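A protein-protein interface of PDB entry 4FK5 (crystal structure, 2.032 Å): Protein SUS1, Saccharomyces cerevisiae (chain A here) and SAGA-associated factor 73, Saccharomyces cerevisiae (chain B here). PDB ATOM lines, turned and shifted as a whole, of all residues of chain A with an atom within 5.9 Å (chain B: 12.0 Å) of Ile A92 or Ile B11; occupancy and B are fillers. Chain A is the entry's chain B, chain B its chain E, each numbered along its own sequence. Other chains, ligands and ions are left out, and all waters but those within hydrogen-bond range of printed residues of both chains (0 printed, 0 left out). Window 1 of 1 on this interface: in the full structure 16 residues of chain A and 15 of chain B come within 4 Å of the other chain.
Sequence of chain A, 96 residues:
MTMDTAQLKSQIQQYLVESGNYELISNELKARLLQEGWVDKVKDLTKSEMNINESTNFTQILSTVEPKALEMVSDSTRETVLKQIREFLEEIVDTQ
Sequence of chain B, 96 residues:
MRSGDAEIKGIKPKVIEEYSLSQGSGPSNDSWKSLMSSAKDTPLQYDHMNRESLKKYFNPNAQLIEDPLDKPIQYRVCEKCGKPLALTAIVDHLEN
Hydrophobic or aromatic side chains of chain B within 4 Å of the printed part of chain A: Ile B8, Ile B11, Pro B13, Val B15, Tyr B19 and Leu B21.
Of the 12 printed residues of chain A, 9 touch a printed residue of chain B.
Hydrophobic or aromatic side chains of chain A that line the printed part of chain B: Leu A8, Ile A12, Tyr A15, Ile A92 and Val A93.
Among the printed residues, Asp or Glu carboxylates within 4 Å of a Lys or Arg side-chain nitrogen of the other chain: Asp A94 with Lys B12 (2.6 Å).
Among the printed residues, pairs that only touch across the chains: Leu A8 with Ile B8 (3.9 Å), Leu A8 with Ile B11 (3.6 Å), Gln A11 with Ile B11 (3.5 Å), Ile A12 with Ile B11 (3.8 Å), Tyr A15 with Val B15 (3.9 Å), Tyr A15 with Tyr B19 (3.6 Å), Glu A91 with Lys B12 (3.4 Å), Ile A92 with Ile B11 (3.4 Å), Ile A92 with Val B15 (3.9 Å), Val A93 with Gly B10 (3.4 Å), Val A93 with Lys B12 (3.6 Å), Asp A94 with Ile B8 (3.6 Å) and Asp A94 with Pro B13 (3.9 Å).
The side-chain amide nitrogen of Gln A7 is in hydrogen-bond range of the backbone carbonyl oxygen of Gln B23, 3.4 Å away.
The side-chain amide oxygen (OE1) of Gln A11 sits close to the backbone carbonyl oxygen (O) of Leu B21, 3.1 Å away.
The backbone NH of Lys B12 is in hydrogen-bond range of the backbone carbonyl oxygen of Ile A92.
The backbone carbonyl oxygen (O) of Asp A94 sits at hydrogen-bond distance from the backbone NH (N) of Lys B9 (2.7 Å).
The backbone carbonyl oxygen (O) of Gly B10 is in hydrogen-bond range of the backbone NH (N) of Asp A94 (2.8 Å).
NZ of Lys B12 lies within salt-bridge range of OD1 of Asp A94 (2.6 Å).
Gln A11 touches just these residues of chain B: Ile B11 and Leu B21.
Of chain B, only Lys B12 (3.4 Å) comes within 4 Å of Glu A91.
Ile A92 touches three residues of chain B.
Printed residues of chain B within 4 Å of Val A93: Gly B10 and Lys B12.
Asp A94 touches just these residues of chain B: Ile B8 (3.6 Å), Lys B9 (2.7 Å), Gly B10 (2.8 Å), Lys B12 (2.6 Å) and Pro B13 (3.9 Å).
Ala B6 touches none of the printed residues of chain A.
Printed residues of chain A within 4 Å of Lys B9: Asp A94.
Ile B11 touches just these residues of chain A: Leu A8 (3.6 Å), Gln A11 (3.5 Å), Ile A12 (3.8 Å) and Ile A92 (3.4 Å).
Lys B14 touches none of the printed residues of chain A.
Of the printed residues of chain A, Val B15 touches Tyr A15 (3.9 Å) and Ile A92 (3.9 Å).
Of the printed residues of chain A, Leu B21 touches Gln A11.
The nearest residue of chain A that does not touch Ile B11 is Val A93 (4.3 Å).
O of Ile B16 sits at hydrogen-bond distance from N of Leu B21 (3.0 Å).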
ATOM      1  N   GLN A   7     -31.355  11.991 -12.206  1.00  0.00           N
ATOM      2  CA  GLN A   7     -32.269  13.032 -11.728  1.00  0.00           C
ATOM      3  C   GLN A   7     -32.029  14.362 -12.496  1.00  0.00           C
ATOM      4  O   GLN A   7     -32.571  15.392 -12.149  1.00  0.00           O
ATOM      5  CB  GLN A   7     -32.087  13.251 -10.230  1.00  0.00           C
ATOM      6  CG  GLN A   7     -30.728  13.822  -9.846  1.00  0.00           C
ATOM      7  CD  GLN A   7     -30.571  14.050  -8.347  1.00  0.00           C
ATOM      8  OE1 GLN A   7     -29.457  14.328  -7.867  1.00  0.00           O
ATOM      9  NE2 GLN A   7     -31.688  13.932  -7.589  1.00  0.00           N
ATOM     10  N   LEU A   8     -31.198  14.297 -13.520  1.00  0.00           N
ATOM     11  CA  LEU A   8     -31.076  15.341 -14.516  1.00  0.00           C
ATOM     12  C   LEU A   8     -32.455  15.846 -14.968  1.00  0.00           C
ATOM     13  O   LEU A   8     -32.703  17.040 -15.019  1.00  0.00           O
ATOM     14  CB  LEU A   8     -30.349  14.776 -15.730  1.00  0.00           C
ATOM     15  CG  LEU A   8     -29.532  15.677 -16.640  1.00  0.00           C
ATOM     16  CD1 LEU A   8     -28.760  16.733 -15.863  1.00  0.00           C
ATOM     17  CD2 LEU A   8     -28.557  14.787 -17.427  1.00  0.00           C
ATOM     18  N   GLN A  11     -34.336  17.807 -12.289  1.00  0.00           N
ATOM     19  CA  GLN A  11     -33.671  19.088 -12.005  1.00  0.00           C
ATOM     20  C   GLN A  11     -33.854  20.084 -13.155  1.00  0.00           C
ATOM     21  O   GLN A  11     -34.019  21.283 -12.915  1.00  0.00           O
ATOM     22  CB  GLN A  11     -32.168  18.893 -11.763  1.00  0.00           C
ATOM     23  CG  GLN A  11     -31.826  18.156 -10.501  1.00  0.00           C
ATOM     24  CD  GLN A  11     -30.304  18.013 -10.339  1.00  0.00           C
ATOM     25  OE1 GLN A  11     -29.774  18.155  -9.233  1.00  0.00           O
ATOM     26  NE2 GLN A  11     -29.595  17.763 -11.457  1.00  0.00           N
ATOM     27  N   ILE A  12     -33.779  19.605 -14.377  1.00  0.00           N
ATOM     28  CA  ILE A  12     -34.073  20.462 -15.553  1.00  0.00           C
ATOM     29  C   ILE A  12     -35.553  20.972 -15.523  1.00  0.00           C
ATOM     30  O   ILE A  12     -35.825  22.163 -15.748  1.00  0.00           O
ATOM     31  CB  ILE A  12     -33.750  19.718 -16.858  1.00  0.00           C
ATOM     32  CG1 ILE A  12     -32.213  19.593 -17.006  1.00  0.00           C
ATOM     33  CG2 ILE A  12     -34.376  20.420 -18.094  1.00  0.00           C
ATOM     34  CD1 ILE A  12     -31.772  18.929 -18.277  1.00  0.00           C
ATOM     35  N   TYR A  15     -35.812  23.723 -12.870  1.00  0.00           N
ATOM     36  CA  TYR A  15     -35.345  24.960 -13.491  1.00  0.00           C
ATOM     37  C   TYR A  15     -36.414  25.561 -14.424  1.00  0.00           C
ATOM     38  O   TYR A  15     -36.705  26.759 -14.371  1.00  0.00           O
ATOM     39  CB  TYR A  15     -34.073  24.735 -14.302  1.00  0.00           C
ATOM     40  CG  TYR A  15     -33.843  25.859 -15.301  1.00  0.00           C
ATOM     41  CD1 TYR A  15     -33.370  27.104 -14.874  1.00  0.00           C
ATOM     42  CD2 TYR A  15     -34.231  25.725 -16.620  1.00  0.00           C
ATOM     43  CE1 TYR A  15     -33.253  28.160 -15.759  1.00  0.00           C
ATOM     44  CE2 TYR A  15     -34.058  26.745 -17.537  1.00  0.00           C
ATOM     45  CZ  TYR A  15     -33.590  27.969 -17.101  1.00  0.00           C
ATOM     46  OH  TYR A  15     -33.512  29.005 -17.964  1.00  0.00           O
ATOM     47  N   PHE A  88     -34.246  26.190 -24.771  1.00  0.00           N
ATOM     48  CA  PHE A  88     -34.164  26.501 -23.349  1.00  0.00           C
ATOM     49  C   PHE A  88     -33.122  25.620 -22.689  1.00  0.00           C
ATOM     50  O   PHE A  88     -32.309  26.100 -21.892  1.00  0.00           O
ATOM     51  CB  PHE A  88     -35.502  26.298 -22.689  1.00  0.00           C
ATOM     52  CG  PHE A  88     -36.489  27.380 -22.949  1.00  0.00           C
ATOM     53  CD1 PHE A  88     -36.199  28.693 -22.611  1.00  0.00           C
ATOM     54  CD2 PHE A  88     -37.757  27.082 -23.410  1.00  0.00           C
ATOM     55  CE1 PHE A  88     -37.121  29.699 -22.825  1.00  0.00           C
ATOM     56  CE2 PHE A  88     -38.728  28.064 -23.527  1.00  0.00           C
ATOM     57  CZ  PHE A  88     -38.417  29.392 -23.222  1.00  0.00           C
ATOM     58  N   LEU A  89     -33.037  24.352 -23.087  1.00  0.00           N
ATOM     59  CA  LEU A  89     -32.025  23.451 -22.436  1.00  0.00           C
ATOM     60  C   LEU A  89     -30.546  23.827 -22.846  1.00  0.00           C
ATOM     61  O   LEU A  89     -29.633  23.770 -22.020  1.00  0.00           O
ATOM     62  CB  LEU A  89     -32.276  21.959 -22.752  1.00  0.00           C
ATOM     63  CG  LEU A  89     -33.575  21.303 -22.326  1.00  0.00           C
ATOM     64  CD1 LEU A  89     -33.457  19.812 -22.070  1.00  0.00           C
ATOM     65  CD2 LEU A  89     -34.294  22.008 -21.190  1.00  0.00           C
ATOM     66  N   GLU A  90     -30.363  24.264 -24.094  1.00  0.00           N
ATOM     67  CA  GLU A  90     -29.047  24.742 -24.592  1.00  0.00           C
ATOM     68  C   GLU A  90     -28.463  25.821 -23.670  1.00  0.00           C
ATOM     69  O   GLU A  90     -27.259  25.892 -23.510  1.00  0.00           O
ATOM     70  CB  GLU A  90     -29.165  25.328 -26.024  1.00  0.00           C
ATOM     71  CG  GLU A  90     -29.078  24.320 -27.169  1.00  0.00           C
ATOM     72  CD  GLU A  90     -29.620  24.896 -28.526  1.00  0.00           C
ATOM     73  OE1 GLU A  90     -30.260  24.134 -29.281  1.00  0.00           O
ATOM     74  OE2 GLU A  90     -29.412  26.122 -28.823  1.00  0.00           O
ATOM     75  N   GLU A  91     -29.324  26.640 -23.067  1.00  0.00           N
ATOM     76  CA  GLU A  91     -28.871  27.697 -22.155  1.00  0.00           C
ATOM     77  C   GLU A  91     -28.323  27.180 -20.837  1.00  0.00           C
ATOM     78  O   GLU A  91     -27.586  27.900 -20.168  1.00  0.00           O
ATOM     79  CB  GLU A  91     -30.008  28.719 -21.851  1.00  0.00           C
ATOM     80  CG  GLU A  91     -30.560  29.407 -23.067  1.00  0.00           C
ATOM     81  CD  GLU A  91     -31.295  30.706 -22.732  1.00  0.00           C
ATOM     82  OE1 GLU A  91     -32.282  30.669 -21.943  1.00  0.00           O
ATOM     83  OE2 GLU A  91     -30.918  31.762 -23.306  1.00  0.00           O
ATOM     84  N   ILE A  92     -28.725  25.974 -20.417  1.00  0.00           N
ATOM     85  CA  ILE A  92     -28.420  25.507 -19.043  1.00  0.00           C
ATOM     86  C   ILE A  92     -27.622  24.196 -18.926  1.00  0.00           C
ATOM     87  O   ILE A  92     -27.279  23.789 -17.795  1.00  0.00           O
ATOM     88  CB  ILE A  92     -29.675  25.379 -18.159  1.00  0.00           C
ATOM     89  CG1 ILE A  92     -30.560  24.199 -18.627  1.00  0.00           C
ATOM     90  CG2 ILE A  92     -30.437  26.716 -18.133  1.00  0.00           C
ATOM     91  CD1 ILE A  92     -31.439  23.625 -17.549  1.00  0.00           C
ATOM     92  N   VAL A  93     -27.371  23.508 -20.035  1.00  0.00           N
ATOM     93  CA  VAL A  93     -26.653  22.242 -19.954  1.00  0.00           C
ATOM     94  C   VAL A  93     -25.293  22.346 -20.674  1.00  0.00           C
ATOM     95  O   VAL A  93     -25.160  23.030 -21.713  1.00  0.00           O
ATOM     96  CB  VAL A  93     -27.492  20.980 -20.490  1.00  0.00           C
ATOM     97  CG1 VAL A  93     -28.957  21.039 -20.070  1.00  0.00           C
ATOM     98  CG2 VAL A  93     -27.371  20.831 -21.977  1.00  0.00           C
ATOM     99  N   ASP A  94     -24.293  21.693 -20.112  1.00  0.00           N
ATOM    100  CA  ASP A  94     -23.014  21.508 -20.822  1.00  0.00           C
ATOM    101  C   ASP A  94     -23.031  20.178 -21.529  1.00  0.00           C
ATOM    102  O   ASP A  94     -23.563  19.183 -20.997  1.00  0.00           O
ATOM    103  CB  ASP A  94     -21.843  21.548 -19.847  1.00  0.00           C
ATOM    104  CG  ASP A  94     -21.718  22.861 -19.160  1.00  0.00           C
ATOM    105  OD1 ASP A  94     -21.761  23.900 -19.880  1.00  0.00           O
ATOM    106  OD2 ASP A  94     -21.607  22.875 -17.894  1.00  0.00           O
ATOM    107  N   ALA B   6     -25.462  15.876 -29.399  1.00  0.00           N
ATOM    108  CA  ALA B   6     -24.361  15.916 -28.400  1.00  0.00           C
ATOM    109  C   ALA B   6     -24.815  15.413 -27.022  1.00  0.00           C
ATOM    110  O   ALA B   6     -25.922  15.723 -26.545  1.00  0.00           O
ATOM    111  CB  ALA B   6     -23.791  17.325 -28.278  1.00  0.00           C
ATOM    112  N   GLU B   7     -23.932  14.671 -26.380  1.00  0.00           N
ATOM    113  CA  GLU B   7     -24.212  14.048 -25.105  1.00  0.00           C
ATOM    114  C   GLU B   7     -24.087  15.050 -23.978  1.00  0.00           C
ATOM    115  O   GLU B   7     -23.201  15.896 -23.986  1.00  0.00           O
ATOM    116  CB  GLU B   7     -23.232  12.900 -24.882  1.00  0.00           C
ATOM    117  CG  GLU B   7     -23.225  12.341 -23.468  1.00  0.00           C
ATOM    118  CD  GLU B   7     -22.296  11.134 -23.319  1.00  0.00           C
ATOM    119  OE1 GLU B   7     -21.522  11.113 -22.356  1.00  0.00           O
ATOM    120  OE2 GLU B   7     -22.365  10.207 -24.163  1.00  0.00           O
ATOM    121  N   ILE B   8     -24.934  14.917 -22.971  1.00  0.00           N
ATOM    122  CA  ILE B   8     -24.950  15.887 -21.866  1.00  0.00           C
ATOM    123  C   ILE B   8     -23.891  15.554 -20.836  1.00  0.00           C
ATOM    124  O   ILE B   8     -23.778  14.423 -20.408  1.00  0.00           O
ATOM    125  CB  ILE B   8     -26.340  15.954 -21.194  1.00  0.00           C
ATOM    126  CG1 ILE B   8     -27.365  16.534 -22.192  1.00  0.00           C
ATOM    127  CG2 ILE B   8     -26.281  16.814 -19.925  1.00  0.00           C
ATOM    128  CD1 ILE B   8     -28.799  16.665 -21.674  1.00  0.00           C
ATOM    129  N   LYS B   9     -23.107  16.557 -20.441  1.00  0.00           N
ATOM    130  CA  LYS B   9     -22.170  16.391 -19.356  1.00  0.00           C
ATOM    131  C   LYS B   9     -22.872  16.625 -18.016  1.00  0.00           C
ATOM    132  O   LYS B   9     -22.769  15.819 -17.104  1.00  0.00           O
ATOM    133  CB  LYS B   9     -20.987  17.351 -19.516  1.00  0.00           C
ATOM    134  CG  LYS B   9     -20.144  17.485 -18.258  1.00  0.00           C
ATOM    135  CD  LYS B   9     -18.865  18.271 -18.514  1.00  0.00           C
ATOM    136  CE  LYS B   9     -17.915  18.192 -17.318  1.00  0.00           C
ATOM    137  NZ  LYS B   9     -16.933  19.310 -17.330  1.00  0.00           N
ATOM    138  N   GLY B  10     -23.598  17.732 -17.918  1.00  0.00           N
ATOM    139  CA  GLY B  10     -24.346  18.061 -16.711  1.00  0.00           C
ATOM    140  C   GLY B  10     -25.068  19.383 -16.911  1.00  0.00           C
ATOM    141  O   GLY B  10     -24.888  20.047 -17.964  1.00  0.00           O
ATOM    142  N   ILE B  11     -25.845  19.782 -15.904  1.00  0.00           N
ATOM    143  CA  ILE B  11     -26.396  21.149 -15.821  1.00  0.00           C
ATOM    144  C   ILE B  11     -25.251  22.107 -15.457  1.00  0.00           C
ATOM    145  O   ILE B  11     -24.406  21.782 -14.624  1.00  0.00           O
ATOM    146  CB  ILE B  11     -27.565  21.227 -14.756  1.00  0.00           C
ATOM    147  CG1 ILE B  11     -28.704  20.242 -15.155  1.00  0.00           C
ATOM    148  CG2 ILE B  11     -28.129  22.655 -14.619  1.00  0.00           C
ATOM    149  CD1 ILE B  11     -29.801  20.063 -14.095  1.00  0.00           C
ATOM    150  N   LYS B  12     -25.179  23.255 -16.118  1.00  0.00           N
ATOM    151  CA  LYS B  12     -24.201  24.284 -15.711  1.00  0.00           C
ATOM    152  C   LYS B  12     -24.230  24.516 -14.182  1.00  0.00           C
ATOM    153  O   LYS B  12     -25.289  24.785 -13.585  1.00  0.00           O
ATOM    154  CB  LYS B  12     -24.425  25.613 -16.450  1.00  0.00           C
ATOM    155  CG  LYS B  12     -24.167  25.553 -17.957  1.00  0.00           C
ATOM    156  CD  LYS B  12     -24.455  26.921 -18.611  1.00  0.00           C
ATOM    157  CE  LYS B  12     -24.330  26.894 -20.128  1.00  0.00           C
ATOM    158  NZ  LYS B  12     -23.294  25.917 -20.585  1.00  0.00           N
ATOM    159  N   PRO B  13     -23.056  24.393 -13.531  1.00  0.00           N
ATOM    160  CA  PRO B  13     -22.941  24.631 -12.108  1.00  0.00           C
ATOM    161  C   PRO B  13     -23.579  25.910 -11.624  1.00  0.00           C
ATOM    162  O   PRO B  13     -24.200  25.941 -10.545  1.00  0.00           O
ATOM    163  CB  PRO B  13     -21.423  24.700 -11.909  1.00  0.00           C
ATOM    164  CG  PRO B  13     -20.891  23.746 -12.941  1.00  0.00           C
ATOM    165  CD  PRO B  13     -21.811  23.816 -14.100  1.00  0.00           C
ATOM    166  N   LYS B  14     -23.434  26.968 -12.396  1.00  0.00           N
ATOM    167  CA  LYS B  14     -24.003  28.234 -12.022  1.00  0.00           C
ATOM    168  C   LYS B  14     -25.526  28.102 -11.922  1.00  0.00           C
ATOM    169  O   LYS B  14     -26.161  28.686 -11.025  1.00  0.00           O
ATOM    170  CB  LYS B  14     -23.623  29.293 -13.042  1.00  0.00           C
ATOM    171  CG  LYS B  14     -24.131  30.685 -12.730  1.00  0.00           C
ATOM    172  CD  LYS B  14     -23.068  31.568 -12.104  1.00  0.00           C
ATOM    173  CE  LYS B  14     -23.664  32.848 -11.520  1.00  0.00           C
ATOM    174  NZ  LYS B  14     -23.975  32.703 -10.067  1.00  0.00           N
ATOM    175  N   VAL B  15     -26.119  27.314 -12.831  1.00  0.00           N
ATOM    176  CA  VAL B  15     -27.593  27.181 -12.853  1.00  0.00           C
ATOM    177  C   VAL B  15     -28.013  26.339 -11.673  1.00  0.00           C
ATOM    178  O   VAL B  15     -28.959  26.665 -10.975  1.00  0.00           O
ATOM    179  CB  VAL B  15     -28.098  26.600 -14.184  1.00  0.00           C
ATOM    180  CG1 VAL B  15     -29.600  26.226 -14.094  1.00  0.00           C
ATOM    181  CG2 VAL B  15     -27.883  27.610 -15.316  1.00  0.00           C
ATOM    182  N   ILE B  16     -27.239  25.307 -11.380  1.00  0.00           N
ATOM    183  CA  ILE B  16     -27.493  24.477 -10.184  1.00  0.00           C
ATOM    184  C   ILE B  16     -27.536  25.353  -8.940  1.00  0.00           C
ATOM    185  O   ILE B  16     -28.416  25.194  -8.099  1.00  0.00           O
ATOM    186  CB  ILE B  16     -26.430  23.375 -10.001  1.00  0.00           C
ATOM    187  CG1 ILE B  16     -26.605  22.255 -11.035  1.00  0.00           C
ATOM    188  CG2 ILE B  16     -26.506  22.776  -8.614  1.00  0.00           C
ATOM    189  CD1 ILE B  16     -25.471  21.231 -10.976  1.00  0.00           C
ATOM    190  N   GLU B  17     -26.606  26.305  -8.846  1.00  0.00           N
ATOM    191  CA  GLU B  17     -26.523  27.162  -7.666  1.00  0.00           C
ATOM    192  C   GLU B  17     -27.647  28.162  -7.646  1.00  0.00           C
ATOM    193  O   GLU B  17     -28.334  28.288  -6.637  1.00  0.00           O
ATOM    194  CB  GLU B  17     -25.186  27.900  -7.608  1.00  0.00           C
ATOM    195  CG  GLU B  17     -24.989  28.728  -6.357  1.00  0.00           C
ATOM    196  CD  GLU B  17     -23.716  29.575  -6.424  1.00  0.00           C
ATOM    197  OE1 GLU B  17     -23.672  30.543  -7.229  1.00  0.00           O
ATOM    198  OE2 GLU B  17     -22.753  29.266  -5.686  1.00  0.00           O
ATOM    199  N   GLU B  18     -27.800  28.927  -8.732  1.00  0.00           N
ATOM    200  CA  GLU B  18     -28.771  29.981  -8.753  1.00  0.00           C
ATOM    201  C   GLU B  18     -30.135  29.425  -8.368  1.00  0.00           C
ATOM    202  O   GLU B  18     -30.926  30.096  -7.730  1.00  0.00           O
ATOM    203  CB  GLU B  18     -28.907  30.617 -10.152  1.00  0.00           C
ATOM    204  CG  GLU B  18     -27.728  31.446 -10.623  1.00  0.00           C
ATOM    205  CD  GLU B  18     -27.789  31.745 -12.139  1.00  0.00           C
ATOM    206  OE1 GLU B  18     -27.072  32.675 -12.598  1.00  0.00           O
ATOM    207  OE2 GLU B  18     -28.541  31.041 -12.879  1.00  0.00           O
ATOM    208  N   TYR B  19     -30.463  28.242  -8.864  1.00  0.00           N
ATOM    209  CA  TYR B  19     -31.838  27.757  -8.735  1.00  0.00           C
ATOM    210  C   TYR B  19     -31.975  26.707  -7.615  1.00  0.00           C
ATOM    211  O   TYR B  19     -33.051  26.175  -7.401  1.00  0.00           O
ATOM    212  CB  TYR B  19     -32.318  27.215 -10.081  1.00  0.00           C
ATOM    213  CG  TYR B  19     -32.712  28.304 -11.046  1.00  0.00           C
ATOM    214  CD1 TYR B  19     -34.014  28.775 -11.082  1.00  0.00           C
ATOM    215  CD2 TYR B  19     -31.791  28.857 -11.936  1.00  0.00           C
ATOM    216  CE1 TYR B  19     -34.379  29.771 -11.928  1.00  0.00           C
ATOM    217  CE2 TYR B  19     -32.161  29.860 -12.809  1.00  0.00           C
ATOM    218  CZ  TYR B  19     -33.471  30.297 -12.800  1.00  0.00           C
ATOM    219  OH  TYR B  19     -33.886  31.264 -13.642  1.00  0.00           O
ATOM    220  N   SER B  20     -30.889  26.476  -6.870  1.00  0.00           N
ATOM    221  CA  SER B  20     -30.850  25.444  -5.785  1.00  0.00           C
ATOM    222  C   SER B  20     -31.355  24.080  -6.215  1.00  0.00           C
ATOM    223  O   SER B  20     -32.177  23.457  -5.507  1.00  0.00           O
ATOM    224  CB  SER B  20     -31.648  25.909  -4.549  1.00  0.00           C
ATOM    225  OG  SER B  20     -31.217  27.199  -4.127  1.00  0.00           O
ATOM    226  N   LEU B  21     -30.861  23.601  -7.352  1.00  0.00           N
ATOM    227  CA  LEU B  21     -31.347  22.342  -7.941  1.00  0.00           C
ATOM    228  C   LEU B  21     -30.880  21.059  -7.185  1.00  0.00           C
ATOM    229  O   LEU B  21     -31.453  20.002  -7.379  1.00  0.00           O
ATOM    230  CB  LEU B  21     -30.922  22.249  -9.404  1.00  0.00           C
ATOM    231  CG  LEU B  21     -31.814  22.814 -10.510  1.00  0.00           C
ATOM    232  CD1 LEU B  21     -32.938  23.723 -10.035  1.00  0.00           C
ATOM    233  CD2 LEU B  21     -30.989  23.473 -11.584  1.00  0.00           C
ATOM    234  N   SER B  22     -29.824  21.140  -6.372  1.00  0.00           N
ATOM    235  CA  SER B  22     -29.367  19.935  -5.608  1.00  0.00           C
ATOM    236  C   SER B  22     -30.426  19.507  -4.592  1.00  0.00           C
ATOM    237  O   SER B  22     -30.700  20.213  -3.628  1.00  0.00           O
ATOM    238  CB  SER B  22     -28.047  20.187  -4.880  1.00  0.00           C
ATOM    239  OG  SER B  22     -27.015  20.504  -5.791  1.00  0.00           O
ATOM    240  N   GLN B  23     -31.028  18.356  -4.834  1.00  0.00           N
ATOM    241  CA  GLN B  23     -32.125  17.872  -4.010  1.00  0.00           C
ATOM    242  C   GLN B  23     -31.874  16.385  -3.684  1.00  0.00           C
ATOM    243  O   GLN B  23     -31.839  15.541  -4.590  1.00  0.00           O
ATOM    244  CB  GLN B  23     -33.479  18.057  -4.756  1.00  0.00           C
ATOM    245  CG  GLN B  23     -33.876  19.530  -5.039  1.00  0.00           C
ATOM    246  CD  GLN B  23     -35.039  19.678  -6.055  1.00  0.00           C
ATOM    247  OE1 GLN B  23     -35.184  20.729  -6.710  1.00  0.00           O
ATOM    248  NE2 GLN B  23     -35.873  18.629  -6.176  1.00  0.00           N
